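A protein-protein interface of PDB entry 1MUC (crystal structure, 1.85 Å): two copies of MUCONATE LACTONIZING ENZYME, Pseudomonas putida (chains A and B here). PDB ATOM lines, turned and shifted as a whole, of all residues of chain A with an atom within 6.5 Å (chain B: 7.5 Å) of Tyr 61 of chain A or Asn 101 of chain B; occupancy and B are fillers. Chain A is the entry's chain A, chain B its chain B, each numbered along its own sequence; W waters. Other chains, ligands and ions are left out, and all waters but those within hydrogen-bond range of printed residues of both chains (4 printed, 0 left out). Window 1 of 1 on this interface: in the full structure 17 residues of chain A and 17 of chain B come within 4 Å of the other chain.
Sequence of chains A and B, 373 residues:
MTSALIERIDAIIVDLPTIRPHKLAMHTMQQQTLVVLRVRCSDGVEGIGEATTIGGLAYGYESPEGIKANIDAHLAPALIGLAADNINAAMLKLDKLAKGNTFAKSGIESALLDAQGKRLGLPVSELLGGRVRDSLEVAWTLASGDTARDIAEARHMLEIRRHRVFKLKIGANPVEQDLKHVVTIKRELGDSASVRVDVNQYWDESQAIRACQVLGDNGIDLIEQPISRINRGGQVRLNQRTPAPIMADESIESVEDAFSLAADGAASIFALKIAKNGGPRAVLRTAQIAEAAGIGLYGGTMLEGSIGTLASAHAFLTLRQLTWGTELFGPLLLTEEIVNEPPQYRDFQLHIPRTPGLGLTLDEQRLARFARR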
ATOM      1  N   THR A  53     -20.404   9.438   5.551  1.00  0.00           N
ATOM      2  CA  THR A  53     -19.328   9.203   4.597  1.00  0.00           C
ATOM      3  C   THR A  53     -19.900   8.412   3.428  1.00  0.00           C
ATOM      4  O   THR A  53     -21.079   8.045   3.438  1.00  0.00           O
ATOM      5  CB  THR A  53     -18.117   8.468   5.223  1.00  0.00           C
ATOM      6  OG1 THR A  53     -17.067   8.352   4.246  1.00  0.00           O
ATOM      7  CG2 THR A  53     -18.512   7.087   5.733  1.00  0.00           C
ATOM      8  N   GLY A  56     -18.857   2.962   3.052  1.00  0.00           N
ATOM      9  CA  GLY A  56     -18.164   2.268   4.125  1.00  0.00           C
ATOM     10  C   GLY A  56     -16.804   2.836   4.485  1.00  0.00           C
ATOM     11  O   GLY A  56     -16.718   3.868   5.139  1.00  0.00           O
ATOM     12  N   LEU A  57     -15.746   2.174   4.027  1.00  0.00           N
ATOM     13  CA  LEU A  57     -14.374   2.576   4.309  1.00  0.00           C
ATOM     14  C   LEU A  57     -13.621   2.970   3.034  1.00  0.00           C
ATOM     15  O   LEU A  57     -12.417   3.217   3.062  1.00  0.00           O
ATOM     16  CB  LEU A  57     -13.657   1.392   4.962  1.00  0.00           C
ATOM     17  CG  LEU A  57     -13.358   1.290   6.457  1.00  0.00           C
ATOM     18  CD1 LEU A  57     -14.164   2.233   7.289  1.00  0.00           C
ATOM     19  CD2 LEU A  57     -13.555  -0.150   6.890  1.00  0.00           C
ATOM     20  N   TYR A  59     -14.016   5.731   1.120  1.00  0.00           N
ATOM     21  CA  TYR A  59     -13.695   7.152   0.987  1.00  0.00           C
ATOM     22  C   TYR A  59     -13.162   7.791   2.266  1.00  0.00           C
ATOM     23  O   TYR A  59     -13.182   9.018   2.415  1.00  0.00           O
ATOM     24  CB  TYR A  59     -14.912   7.925   0.460  1.00  0.00           C
ATOM     25  CG  TYR A  59     -15.294   7.563  -0.965  1.00  0.00           C
ATOM     26  CD1 TYR A  59     -15.922   6.351  -1.255  1.00  0.00           C
ATOM     27  CD2 TYR A  59     -14.997   8.419  -2.027  1.00  0.00           C
ATOM     28  CE1 TYR A  59     -16.250   6.000  -2.566  1.00  0.00           C
ATOM     29  CE2 TYR A  59     -15.319   8.083  -3.342  1.00  0.00           C
ATOM     30  CZ  TYR A  59     -15.940   6.871  -3.603  1.00  0.00           C
ATOM     31  OH  TYR A  59     -16.254   6.531  -4.902  1.00  0.00           O
ATOM     32  N   GLY A  60     -12.650   6.961   3.169  1.00  0.00           N
ATOM     33  CA  GLY A  60     -12.116   7.462   4.424  1.00  0.00           C
ATOM     34  C   GLY A  60     -11.898   6.344   5.430  1.00  0.00           C
ATOM     35  O   GLY A  60     -12.320   5.213   5.211  1.00  0.00           O
ATOM     36  N   TYR A  61     -11.266   6.683   6.550  1.00  0.00           N
ATOM     37  CA  TYR A  61     -10.957   5.727   7.613  1.00  0.00           C
ATOM     38  C   TYR A  61     -12.147   5.322   8.474  1.00  0.00           C
ATOM     39  O   TYR A  61     -12.128   4.264   9.106  1.00  0.00           O
ATOM     40  CB  TYR A  61      -9.911   6.336   8.556  1.00  0.00           C
ATOM     41  CG  TYR A  61      -8.705   6.905   7.862  1.00  0.00           C
ATOM     42  CD1 TYR A  61      -7.991   6.142   6.941  1.00  0.00           C
ATOM     43  CD2 TYR A  61      -8.260   8.200   8.136  1.00  0.00           C
ATOM     44  CE1 TYR A  61      -6.859   6.642   6.311  1.00  0.00           C
ATOM     45  CE2 TYR A  61      -7.121   8.712   7.507  1.00  0.00           C
ATOM     46  CZ  TYR A  61      -6.425   7.919   6.596  1.00  0.00           C
ATOM     47  OH  TYR A  61      -5.275   8.371   5.987  1.00  0.00           O
ATOM     48  N   GLU A  62     -13.137   6.208   8.556  1.00  0.00           N
ATOM     49  CA  GLU A  62     -14.315   6.008   9.393  1.00  0.00           C
ATOM     50  C   GLU A  62     -15.546   5.541   8.644  1.00  0.00           C
ATOM     51  O   GLU A  62     -15.961   6.160   7.666  1.00  0.00           O
ATOM     52  CB  GLU A  62     -14.651   7.310  10.135  1.00  0.00           C
ATOM     53  CG  GLU A  62     -13.519   7.825  11.030  1.00  0.00           C
ATOM     54  CD  GLU A  62     -13.765   9.238  11.524  1.00  0.00           C
ATOM     55  OE1 GLU A  62     -14.570   9.424  12.454  1.00  0.00           O
ATOM     56  OE2 GLU A  62     -13.163  10.175  10.973  1.00  0.00           O
ATOM     57  N   SER A  63     -16.144   4.464   9.143  1.00  0.00           N
ATOM     58  CA  SER A  63     -17.356   3.900   8.561  1.00  0.00           C
ATOM     59  C   SER A  63     -18.481   4.273   9.526  1.00  0.00           C
ATOM     60  O   SER A  63     -18.201   4.687  10.657  1.00  0.00           O
ATOM     61  CB  SER A  63     -17.232   2.381   8.488  1.00  0.00           C
ATOM     62  OG  SER A  63     -17.137   1.838   9.791  1.00  0.00           O
ATOM     63  N   PHE A 103     -14.743  12.741  11.257  1.00  0.00           N
ATOM     64  CA  PHE A 103     -16.163  12.639  10.907  1.00  0.00           C
ATOM     65  C   PHE A 103     -16.995  12.662  12.190  1.00  0.00           C
ATOM     66  O   PHE A 103     -17.991  13.378  12.271  1.00  0.00           O
ATOM     67  CB  PHE A 103     -16.462  11.340  10.146  1.00  0.00           C
ATOM     68  CG  PHE A 103     -16.006  11.344   8.705  1.00  0.00           C
ATOM     69  CD1 PHE A 103     -14.652  11.390   8.383  1.00  0.00           C
ATOM     70  CD2 PHE A 103     -16.930  11.285   7.673  1.00  0.00           C
ATOM     71  CE1 PHE A 103     -14.234  11.381   7.058  1.00  0.00           C
ATOM     72  CE2 PHE A 103     -16.512  11.277   6.340  1.00  0.00           C
ATOM     73  CZ  PHE A 103     -15.172  11.325   6.037  1.00  0.00           C
ATOM     74  N   ARG A 229      -3.007  11.272  -2.900  1.00  0.00           N
ATOM     75  CA  ARG A 229      -2.407  12.157  -1.903  1.00  0.00           C
ATOM     76  C   ARG A 229      -1.014  11.708  -1.483  1.00  0.00           C
ATOM     77  O   ARG A 229      -0.269  12.489  -0.908  1.00  0.00           O
ATOM     78  CB  ARG A 229      -3.293  12.252  -0.666  1.00  0.00           C
ATOM     79  CG  ARG A 229      -3.415  10.951   0.092  1.00  0.00           C
ATOM     80  CD  ARG A 229      -4.557  10.992   1.085  1.00  0.00           C
ATOM     81  NE  ARG A 229      -4.434  12.129   1.989  1.00  0.00           N
ATOM     82  CZ  ARG A 229      -3.565  12.198   2.991  1.00  0.00           C
ATOM     83  NH1 ARG A 229      -2.733  11.189   3.231  1.00  0.00           N
ATOM     84  NH2 ARG A 229      -3.515  13.292   3.737  1.00  0.00           N
ATOM     85  N   GLU A 253      -6.849  15.774   4.962  1.00  0.00           N
ATOM     86  CA  GLU A 253      -7.481  14.897   5.947  1.00  0.00           C
ATOM     87  C   GLU A 253      -7.412  15.508   7.330  1.00  0.00           C
ATOM     88  O   GLU A 253      -7.726  14.852   8.314  1.00  0.00           O
ATOM     89  CB  GLU A 253      -6.813  13.528   5.961  1.00  0.00           C
ATOM     90  CG  GLU A 253      -7.184  12.703   4.765  1.00  0.00           C
ATOM     91  CD  GLU A 253      -6.551  11.329   4.781  1.00  0.00           C
ATOM     92  OE1 GLU A 253      -5.735  11.046   5.679  1.00  0.00           O
ATOM     93  OE2 GLU A 253      -6.877  10.531   3.883  1.00  0.00           O
ATOM     94  N   LYS A 276     -13.859  16.070   6.883  1.00  0.00           N
ATOM     95  CA  LYS A 276     -12.432  15.774   6.749  1.00  0.00           C
ATOM     96  C   LYS A 276     -11.557  16.605   7.670  1.00  0.00           C
ATOM     97  O   LYS A 276     -10.376  16.304   7.865  1.00  0.00           O
ATOM     98  CB  LYS A 276     -11.978  16.008   5.306  1.00  0.00           C
ATOM     99  CG  LYS A 276     -12.835  15.343   4.244  1.00  0.00           C
ATOM    100  CD  LYS A 276     -12.719  13.833   4.245  1.00  0.00           C
ATOM    101  CE  LYS A 276     -11.350  13.363   3.799  1.00  0.00           C
ATOM    102  NZ  LYS A 276     -11.409  11.910   3.467  1.00  0.00           N
ATOM    103  N   TYR B  61      -5.880   6.250  15.421  1.00  0.00           N
ATOM    104  CA  TYR B  61      -7.233   6.408  14.901  1.00  0.00           C
ATOM    105  C   TYR B  61      -8.161   5.240  15.251  1.00  0.00           C
ATOM    106  O   TYR B  61      -9.382   5.410  15.308  1.00  0.00           O
ATOM    107  CB  TYR B  61      -7.184   6.539  13.372  1.00  0.00           C
ATOM    108  CG  TYR B  61      -6.238   7.606  12.872  1.00  0.00           C
ATOM    109  CD1 TYR B  61      -6.151   8.845  13.510  1.00  0.00           C
ATOM    110  CD2 TYR B  61      -5.438   7.385  11.752  1.00  0.00           C
ATOM    111  CE1 TYR B  61      -5.290   9.842  13.043  1.00  0.00           C
ATOM    112  CE2 TYR B  61      -4.573   8.376  11.276  1.00  0.00           C
ATOM    113  CZ  TYR B  61      -4.508   9.604  11.926  1.00  0.00           C
ATOM    114  OH  TYR B  61      -3.684  10.608  11.454  1.00  0.00           O
ATOM    115  N   GLU B  62      -7.582   4.050  15.429  1.00  0.00           N
ATOM    116  CA  GLU B  62      -8.346   2.831  15.714  1.00  0.00           C
ATOM    117  C   GLU B  62      -8.369   2.387  17.170  1.00  0.00           C
ATOM    118  O   GLU B  62      -7.325   2.257  17.804  1.00  0.00           O
ATOM    119  CB  GLU B  62      -7.828   1.670  14.853  1.00  0.00           C
ATOM    120  CG  GLU B  62      -7.915   1.919  13.370  1.00  0.00           C
ATOM    121  CD  GLU B  62      -7.128   0.900  12.572  1.00  0.00           C
ATOM    122  OE1 GLU B  62      -7.654  -0.212  12.341  1.00  0.00           O
ATOM    123  OE2 GLU B  62      -5.985   1.213  12.174  1.00  0.00           O
ATOM    124  N   GLY B  66     -13.769   0.095  17.481  1.00  0.00           N
ATOM    125  CA  GLY B  66     -13.859   0.438  16.069  1.00  0.00           C
ATOM    126  C   GLY B  66     -13.241  -0.654  15.210  1.00  0.00           C
ATOM    127  O   GLY B  66     -13.750  -0.954  14.129  1.00  0.00           O
ATOM    128  N   ILE B  67     -12.137  -1.237  15.677  1.00  0.00           N
ATOM    129  CA  ILE B  67     -11.453  -2.325  14.961  1.00  0.00           C
ATOM    130  C   ILE B  67     -12.380  -3.524  14.782  1.00  0.00           C
ATOM    131  O   ILE B  67     -12.512  -4.057  13.675  1.00  0.00           O
ATOM    132  CB  ILE B  67     -10.172  -2.771  15.710  1.00  0.00           C
ATOM    133  CG1 ILE B  67      -9.062  -1.739  15.500  1.00  0.00           C
ATOM    134  CG2 ILE B  67      -9.727  -4.154  15.242  1.00  0.00           C
ATOM    135  CD1 ILE B  67      -7.944  -1.819  16.537  1.00  0.00           C
ATOM    136  N   ASN B  70     -15.382  -2.674  12.365  1.00  0.00           N
ATOM    137  CA  ASN B  70     -15.012  -2.652  10.963  1.00  0.00           C
ATOM    138  C   ASN B  70     -14.688  -4.010  10.404  1.00  0.00           C
ATOM    139  O   ASN B  70     -14.989  -4.275   9.245  1.00  0.00           O
ATOM    140  CB  ASN B  70     -13.874  -1.667  10.719  1.00  0.00           C
ATOM    141  CG  ASN B  70     -14.354  -0.237  10.765  1.00  0.00           C
ATOM    142  OD1 ASN B  70     -15.383   0.086  10.175  1.00  0.00           O
ATOM    143  ND2 ASN B  70     -13.641   0.619  11.484  1.00  0.00           N
ATOM    144  N   ILE B  71     -14.068  -4.872  11.205  1.00  0.00           N
ATOM    145  CA  ILE B  71     -13.748  -6.217  10.737  1.00  0.00           C
ATOM    146  C   ILE B  71     -15.032  -6.971  10.453  1.00  0.00           C
ATOM    147  O   ILE B  71     -15.209  -7.512   9.368  1.00  0.00           O
ATOM    148  CB  ILE B  71     -12.902  -7.005  11.754  1.00  0.00           C
ATOM    149  CG1 ILE B  71     -11.465  -6.481  11.738  1.00  0.00           C
ATOM    150  CG2 ILE B  71     -12.918  -8.504  11.428  1.00  0.00           C
ATOM    151  CD1 ILE B  71     -10.567  -7.105  12.770  1.00  0.00           C
ATOM    152  N   LEU B  75     -14.469  -5.562   6.592  1.00  0.00           N
ATOM    153  CA  LEU B  75     -13.288  -6.316   6.198  1.00  0.00           C
ATOM    154  C   LEU B  75     -13.498  -7.818   6.043  1.00  0.00           C
ATOM    155  O   LEU B  75     -13.248  -8.363   4.971  1.00  0.00           O
ATOM    156  CB  LEU B  75     -12.121  -5.980   7.135  1.00  0.00           C
ATOM    157  CG  LEU B  75     -11.755  -4.477   7.201  1.00  0.00           C
ATOM    158  CD1 LEU B  75     -10.660  -4.251   8.238  1.00  0.00           C
ATOM    159  CD2 LEU B  75     -11.301  -3.951   5.832  1.00  0.00           C
ATOM    160  N   MET B  91      -4.896  -9.040   0.776  1.00  0.00           N
ATOM    161  CA  MET B  91      -4.554  -7.735   1.329  1.00  0.00           C
ATOM    162  C   MET B  91      -4.742  -6.589   0.331  1.00  0.00           C
ATOM    163  O   MET B  91      -5.075  -5.473   0.730  1.00  0.00           O
ATOM    164  CB  MET B  91      -3.137  -7.742   1.900  1.00  0.00           C
ATOM    165  CG  MET B  91      -2.901  -8.804   2.987  1.00  0.00           C
ATOM    166  SD  MET B  91      -4.130  -8.821   4.305  1.00  0.00           S
ATOM    167  CE  MET B  91      -4.008  -7.093   4.949  1.00  0.00           C
ATOM    168  N   LEU B  94      -8.296  -5.659   0.369  1.00  0.00           N
ATOM    169  CA  LEU B  94      -8.610  -4.831   1.527  1.00  0.00           C
ATOM    170  C   LEU B  94      -8.162  -3.387   1.316  1.00  0.00           C
ATOM    171  O   LEU B  94      -8.833  -2.470   1.757  1.00  0.00           O
ATOM    172  CB  LEU B  94      -7.998  -5.408   2.809  1.00  0.00           C
ATOM    173  CG  LEU B  94      -8.542  -6.770   3.250  1.00  0.00           C
ATOM    174  CD1 LEU B  94      -7.904  -7.181   4.562  1.00  0.00           C
ATOM    175  CD2 LEU B  94     -10.055  -6.712   3.407  1.00  0.00           C
ATOM    176  N   ASP B  95      -7.043  -3.181   0.621  1.00  0.00           N
ATOM    177  CA  ASP B  95      -6.557  -1.813   0.363  1.00  0.00           C
ATOM    178  C   ASP B  95      -7.499  -1.085  -0.584  1.00  0.00           C
ATOM    179  O   ASP B  95      -7.695   0.126  -0.475  1.00  0.00           O
ATOM    180  CB  ASP B  95      -5.147  -1.828  -0.234  1.00  0.00           C
ATOM    181  CG  ASP B  95      -4.050  -1.891   0.832  1.00  0.00           C
ATOM    182  OD1 ASP B  95      -4.354  -1.757   2.044  1.00  0.00           O
ATOM    183  OD2 ASP B  95      -2.869  -2.064   0.455  1.00  0.00           O
ATOM    184  N   LEU B  97     -10.815  -1.648  -0.877  1.00  0.00           N
ATOM    185  CA  LEU B  97     -12.077  -1.367  -0.203  1.00  0.00           C
ATOM    186  C   LEU B  97     -11.970  -0.517   1.046  1.00  0.00           C
ATOM    187  O   LEU B  97     -12.956   0.103   1.443  1.00  0.00           O
ATOM    188  CB  LEU B  97     -12.790  -2.675   0.155  1.00  0.00           C
ATOM    189  CG  LEU B  97     -13.589  -3.372  -0.951  1.00  0.00           C
ATOM    190  CD1 LEU B  97     -12.771  -3.545  -2.234  1.00  0.00           C
ATOM    191  CD2 LEU B  97     -14.078  -4.712  -0.425  1.00  0.00           C
ATOM    192  N   ALA B  98     -10.785  -0.450   1.650  1.00  0.00           N
ATOM    193  CA  ALA B  98     -10.634   0.293   2.894  1.00  0.00           C
ATOM    194  C   ALA B  98      -9.420   1.176   2.967  1.00  0.00           C
ATOM    195  O   ALA B  98      -8.294   0.728   2.738  1.00  0.00           O
ATOM    196  CB  ALA B  98     -10.622  -0.673   4.065  1.00  0.00           C
ATOM    197  N   LYS B  99      -9.652   2.435   3.307  1.00  0.00           N
ATOM    198  CA  LYS B  99      -8.566   3.382   3.447  1.00  0.00           C
ATOM    199  C   LYS B  99      -8.040   3.269   4.871  1.00  0.00           C
ATOM    200  O   LYS B  99      -8.819   3.165   5.816  1.00  0.00           O
ATOM    201  CB  LYS B  99      -9.066   4.809   3.174  1.00  0.00           C
ATOM    202  CG  LYS B  99      -9.491   5.039   1.723  1.00  0.00           C
ATOM    203  CD  LYS B  99      -8.287   4.942   0.776  1.00  0.00           C
ATOM    204  CE  LYS B  99      -8.689   4.558  -0.652  1.00  0.00           C
ATOM    205  NZ  LYS B  99      -9.087   3.119  -0.802  1.00  0.00           N
ATOM    206  N   GLY B 100      -6.723   3.239   5.027  1.00  0.00           N
ATOM    207  CA  GLY B 100      -6.174   3.172   6.363  1.00  0.00           C
ATOM    208  C   GLY B 100      -6.549   1.880   7.050  1.00  0.00           C
ATOM    209  O   GLY B 100      -6.481   0.830   6.441  1.00  0.00           O
ATOM    210  N   ASN B 101      -6.962   1.954   8.309  1.00  0.00           N
ATOM    211  CA  ASN B 101      -7.323   0.759   9.073  1.00  0.00           C
ATOM    212  C   ASN B 101      -6.146  -0.220   9.117  1.00  0.00           C
ATOM    213  O   ASN B 101      -6.319  -1.423   9.001  1.00  0.00           O
ATOM    214  CB  ASN B 101      -8.591   0.110   8.498  1.00  0.00           C
ATOM    215  CG  ASN B 101      -9.844   0.912   8.824  1.00  0.00           C
ATOM    216  OD1 ASN B 101     -10.510   0.644   9.811  1.00  0.00           O
ATOM    217  ND2 ASN B 101     -10.141   1.927   8.016  1.00  0.00           N
ATOM    218  N   THR B 102      -4.949   0.311   9.347  1.00  0.00           N
ATOM    219  CA  THR B 102      -3.733  -0.496   9.390  1.00  0.00           C
ATOM    220  C   THR B 102      -3.690  -1.509  10.549  1.00  0.00           C
ATOM    221  O   THR B 102      -3.140  -2.601  10.394  1.00  0.00           O
ATOM    222  CB  THR B 102      -2.470   0.406   9.406  1.00  0.00           C
ATOM    223  OG1 THR B 102      -2.562   1.340  10.487  1.00  0.00           O
ATOM    224  CG2 THR B 102      -2.345   1.174   8.109  1.00  0.00           C
ATOM    225  N   PHE B 103      -4.273  -1.160  11.698  1.00  0.00           N
ATOM    226  CA  PHE B 103      -4.291  -2.083  12.838  1.00  0.00           C
ATOM    227  C   PHE B 103      -5.129  -3.320  12.497  1.00  0.00           C
ATOM    228  O   PHE B 103      -4.696  -4.458  12.705  1.00  0.00           O
ATOM    229  CB  PHE B 103      -4.840  -1.413  14.106  1.00  0.00           C
ATOM    230  CG  PHE B 103      -3.885  -0.451  14.753  1.00  0.00           C
ATOM    231  CD1 PHE B 103      -3.501   0.718  14.102  1.00  0.00           C
ATOM    232  CD2 PHE B 103      -3.366  -0.715  16.017  1.00  0.00           C
ATOM    233  CE1 PHE B 103      -2.621   1.605  14.695  1.00  0.00           C
ATOM    234  CE2 PHE B 103      -2.480   0.168  16.628  1.00  0.00           C
ATOM    235  CZ  PHE B 103      -2.107   1.337  15.957  1.00  0.00           C
ATOM    236  N   ALA B 104      -6.328  -3.092  11.979  1.00  0.00           N
ATOM    237  CA  ALA B 104      -7.205  -4.178  11.595  1.00  0.00           C
ATOM    238  C   ALA B 104      -6.524  -4.997  10.499  1.00  0.00           C
ATOM    239  O   ALA B 104      -6.518  -6.216  10.559  1.00  0.00           O
ATOM    240  CB  ALA B 104      -8.534  -3.629  11.109  1.00  0.00           C
ATOM    241  N   LYS B 105      -5.936  -4.325   9.510  1.00  0.00           N
ATOM    242  CA  LYS B 105      -5.245  -5.014   8.412  1.00  0.00           C
ATOM    243  C   LYS B 105      -4.082  -5.864   8.913  1.00  0.00           C
ATOM    244  O   LYS B 105      -3.881  -6.991   8.451  1.00  0.00           O
ATOM    245  CB  LYS B 105      -4.752  -4.007   7.371  1.00  0.00           C
ATOM    246  CG  LYS B 105      -5.860  -3.496   6.484  1.00  0.00           C
ATOM    247  CD  LYS B 105      -5.404  -2.330   5.641  1.00  0.00           C
ATOM    248  CE  LYS B 105      -6.540  -1.823   4.766  1.00  0.00           C
ATOM    249  NZ  LYS B 105      -6.134  -0.586   4.036  1.00  0.00           N
ATOM    250  N   SER B 106      -3.323  -5.315   9.856  1.00  0.00           N
ATOM    251  CA  SER B 106      -2.186  -5.999  10.460  1.00  0.00           C
ATOM    252  C   SER B 106      -2.624  -7.292  11.157  1.00  0.00           C
ATOM    253  O   SER B 106      -1.946  -8.317  11.067  1.00  0.00           O
ATOM    254  CB  SER B 106      -1.534  -5.088  11.487  1.00  0.00           C
ATOM    255  OG  SER B 106      -0.463  -5.760  12.133  1.00  0.00           O
ATOM    256  N   GLY B 107      -3.737  -7.217  11.883  1.00  0.00           N
ATOM    257  CA  GLY B 107      -4.251  -8.373  12.590  1.00  0.00           C
ATOM    258  C   GLY B 107      -4.665  -9.449  11.607  1.00  0.00           C
ATOM    259  O   GLY B 107      -4.355 -10.616  11.788  1.00  0.00           O
ATOM    260  N   ILE B 108      -5.322  -9.045  10.530  1.00  0.00           N
ATOM    261  CA  ILE B 108      -5.764  -9.985   9.516  1.00  0.00           C
ATOM    262  C   ILE B 108      -4.607 -10.615   8.745  1.00  0.00           C
ATOM    263  O   ILE B 108      -4.632 -11.817   8.479  1.00  0.00           O
ATOM    264  CB  ILE B 108      -6.767  -9.314   8.550  1.00  0.00           C
ATOM    265  CG1 ILE B 108      -8.085  -9.075   9.273  1.00  0.00           C
ATOM    266  CG2 ILE B 108      -7.003 -10.172   7.310  1.00  0.00           C
ATOM    267  CD1 ILE B 108      -9.017  -8.181   8.521  1.00  0.00           C
ATOM    268  N   GLU B 253       2.597   6.580   9.639  1.00  0.00           N
ATOM    269  CA  GLU B 253       1.262   6.021   9.792  1.00  0.00           C
ATOM    270  C   GLU B 253       0.897   5.202   8.572  1.00  0.00           C
ATOM    271  O   GLU B 253      -0.243   4.793   8.413  1.00  0.00           O
ATOM    272  CB  GLU B 253       0.233   7.126   9.981  1.00  0.00           C
ATOM    273  CG  GLU B 253       0.373   7.859  11.299  1.00  0.00           C
ATOM    274  CD  GLU B 253      -0.794   8.804  11.546  1.00  0.00           C
ATOM    275  OE1 GLU B 253      -1.490   9.174  10.579  1.00  0.00           O
ATOM    276  OE2 GLU B 253      -1.019   9.179  12.710  1.00  0.00           O
ATOM    277  N   SER B 254       1.866   5.022   7.679  1.00  0.00           N
ATOM    278  CA  SER B 254       1.677   4.237   6.472  1.00  0.00           C
ATOM    279  C   SER B 254       3.035   4.085   5.805  1.00  0.00           C
ATOM    280  O   SER B 254       3.972   4.816   6.122  1.00  0.00           O
ATOM    281  CB  SER B 254       0.710   4.937   5.520  1.00  0.00           C
ATOM    282  OG  SER B 254       1.304   6.106   4.992  1.00  0.00           O
ATOM    283  N   ALA B 275       1.514  -2.680  13.188  1.00  0.00           N
ATOM    284  CA  ALA B 275       0.199  -2.051  13.369  1.00  0.00           C
ATOM    285  C   ALA B 275       0.014  -0.706  12.647  1.00  0.00           C
ATOM    286  O   ALA B 275      -1.091  -0.394  12.202  1.00  0.00           O
ATOM    287  CB  ALA B 275      -0.097  -1.896  14.863  1.00  0.00           C
ATOM    288  N   ASN B 277       1.714   0.140   9.928  1.00  0.00           N
ATOM    289  CA  ASN B 277       1.970  -0.083   8.509  1.00  0.00           C
ATOM    290  C   ASN B 277       0.951  -0.966   7.822  1.00  0.00           C
ATOM    291  O   ASN B 277       0.689  -0.804   6.634  1.00  0.00           O
ATOM    292  CB  ASN B 277       3.391  -0.627   8.308  1.00  0.00           C
ATOM    293  CG  ASN B 277       4.435   0.422   8.572  1.00  0.00           C
ATOM    294  OD1 ASN B 277       4.975   0.528   9.672  1.00  0.00           O
ATOM    295  ND2 ASN B 277       4.660   1.259   7.595  1.00  0.00           N
ATOM    296  N   GLY B 278       0.382  -1.908   8.563  1.00  0.00           N
ATOM    297  CA  GLY B 278      -0.612  -2.783   7.976  1.00  0.00           C
ATOM    298  C   GLY B 278      -0.286  -4.263   7.996  1.00  0.00           C
ATOM    299  O   GLY B 278      -0.874  -5.023   7.231  1.00  0.00           O
HETATM  300  O   HOH W   1     -14.488   3.380  11.324  1.00  0.00           O
HETATM  301  O   HOH W   2     -15.808  -0.563   2.696  1.00  0.00           O
HETATM  302  O   HOH W   3      -2.542   8.491   8.101  1.00  0.00           O
HETATM  303  O   HOH W   4     -10.713   3.531  11.512  1.00  0.00           O
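O of Leu 57 of chain A lies within hydrogen-bond range of N of Lys 99 of chain B, at 2.9 Å. ND2 of Asn 101 of chain B sits at hydrogen-bond distance from O of Tyr 61 of chain A, 3.3 Å away. The side-chain hydroxyl (OG) of Ser 63 of chain A sits at hydrogen-bond distance from the side-chain amide oxygen (OD1) of Asn 70 of chain B (2.5 Å).
Water W4 bridges O of Tyr 61 of chain A (2.9 Å) and OD1 of Asn 101 of chain B (3.4 Å). Water W1 lies within hydrogen-bond range of the side-chain amide nitrogen (ND2) of Asn 70 of chain B, the backbone NH (N) of Ser 63 of chain A and the backbone carbonyl oxygen (O) of Tyr 61 of chain A. Water W2 bridges the backbone NH (N) of Leu 57 of chain A and the backbone carbonyl oxygen (O) of Leu 97 of chain B.
Positions printed for both chains: 61, 62, 103 and 253.
ND2 of Asn 70 of chain B sits at hydrogen-bond distance from O of Gly 66 of chain B (3.1 Å). OH of Tyr 61 of chain A sits at hydrogen-bond distance from OE1 of Glu 253 of chain A (2.7 Å). The backbone carbonyl oxygen of Gly 100 of chain B is in hydrogen-bond range of the side-chain amino group of Lys 105 of chain B (2.8 Å).
CD2 of Leu 57 of chain A touches OD1 of Asn 70 of chain B (3.8 Å). Leu 97 of chain B touches Leu 57 of chain A. O of Leu 57 of chain A touches CA of Ala 98 of chain B (3.4 Å). CG of Leu 57 of chain A touches ND2 of Asn 101 of chain B (3.6 Å). Lys 99 of chain B touches Gly 60 of chain A. O of Lys 99 of chain B touches CD1 of Tyr 61 of chain A, 3.3 Å away. Tyr 61 of chain A touches Gly 100 of chain B.
Hydrophobic or aromatic side chains of chain B within 4 Å of the printed part of chain A: Ala 98. Of the 12 printed residues of chain A, 4 touch a printed residue of chain B. Printed residues of chain A that touch a printed residue of chain B: Leu 57, Gly 60, Tyr 61 and Ser 63. Among the printed residues, no Asp or Glu carboxylate lies within 4 Å of a Lys or Arg side-chain nitrogen of the other chain.
Of the printed residues of chain B, Gly 60 of chain A touches Lys 99 (3.9 Å). Of chain B, only Lys 99, Gly 100 and Asn 101 come within 4 Å of Tyr 61 of chain A. Glu 62 of chain B touches none of the printed residues of chain A. Of the printed residues of chain A, Asn 70 of chain B touches Leu 57 and Ser 63. Printed residues of chain A within 4 Å of Lys 99 of chain B: Leu 57, Gly 60 and Tyr 61. Printed residues of chain A within 4 Å of Gly 100 of chain B: Tyr 61 (3.5 Å). The nearest residue of chain B that does not touch Tyr 61 of chain A is Tyr 61 of chain B (4.6 Å). The nearest residue of chain A that does not touch Asn 101 of chain B is Gly 60 of chain A (4.8 Å). The nearest printed residue of chain B that does not touch Ser 63 of chain A is Gly 66 of chain B (6.2 Å).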
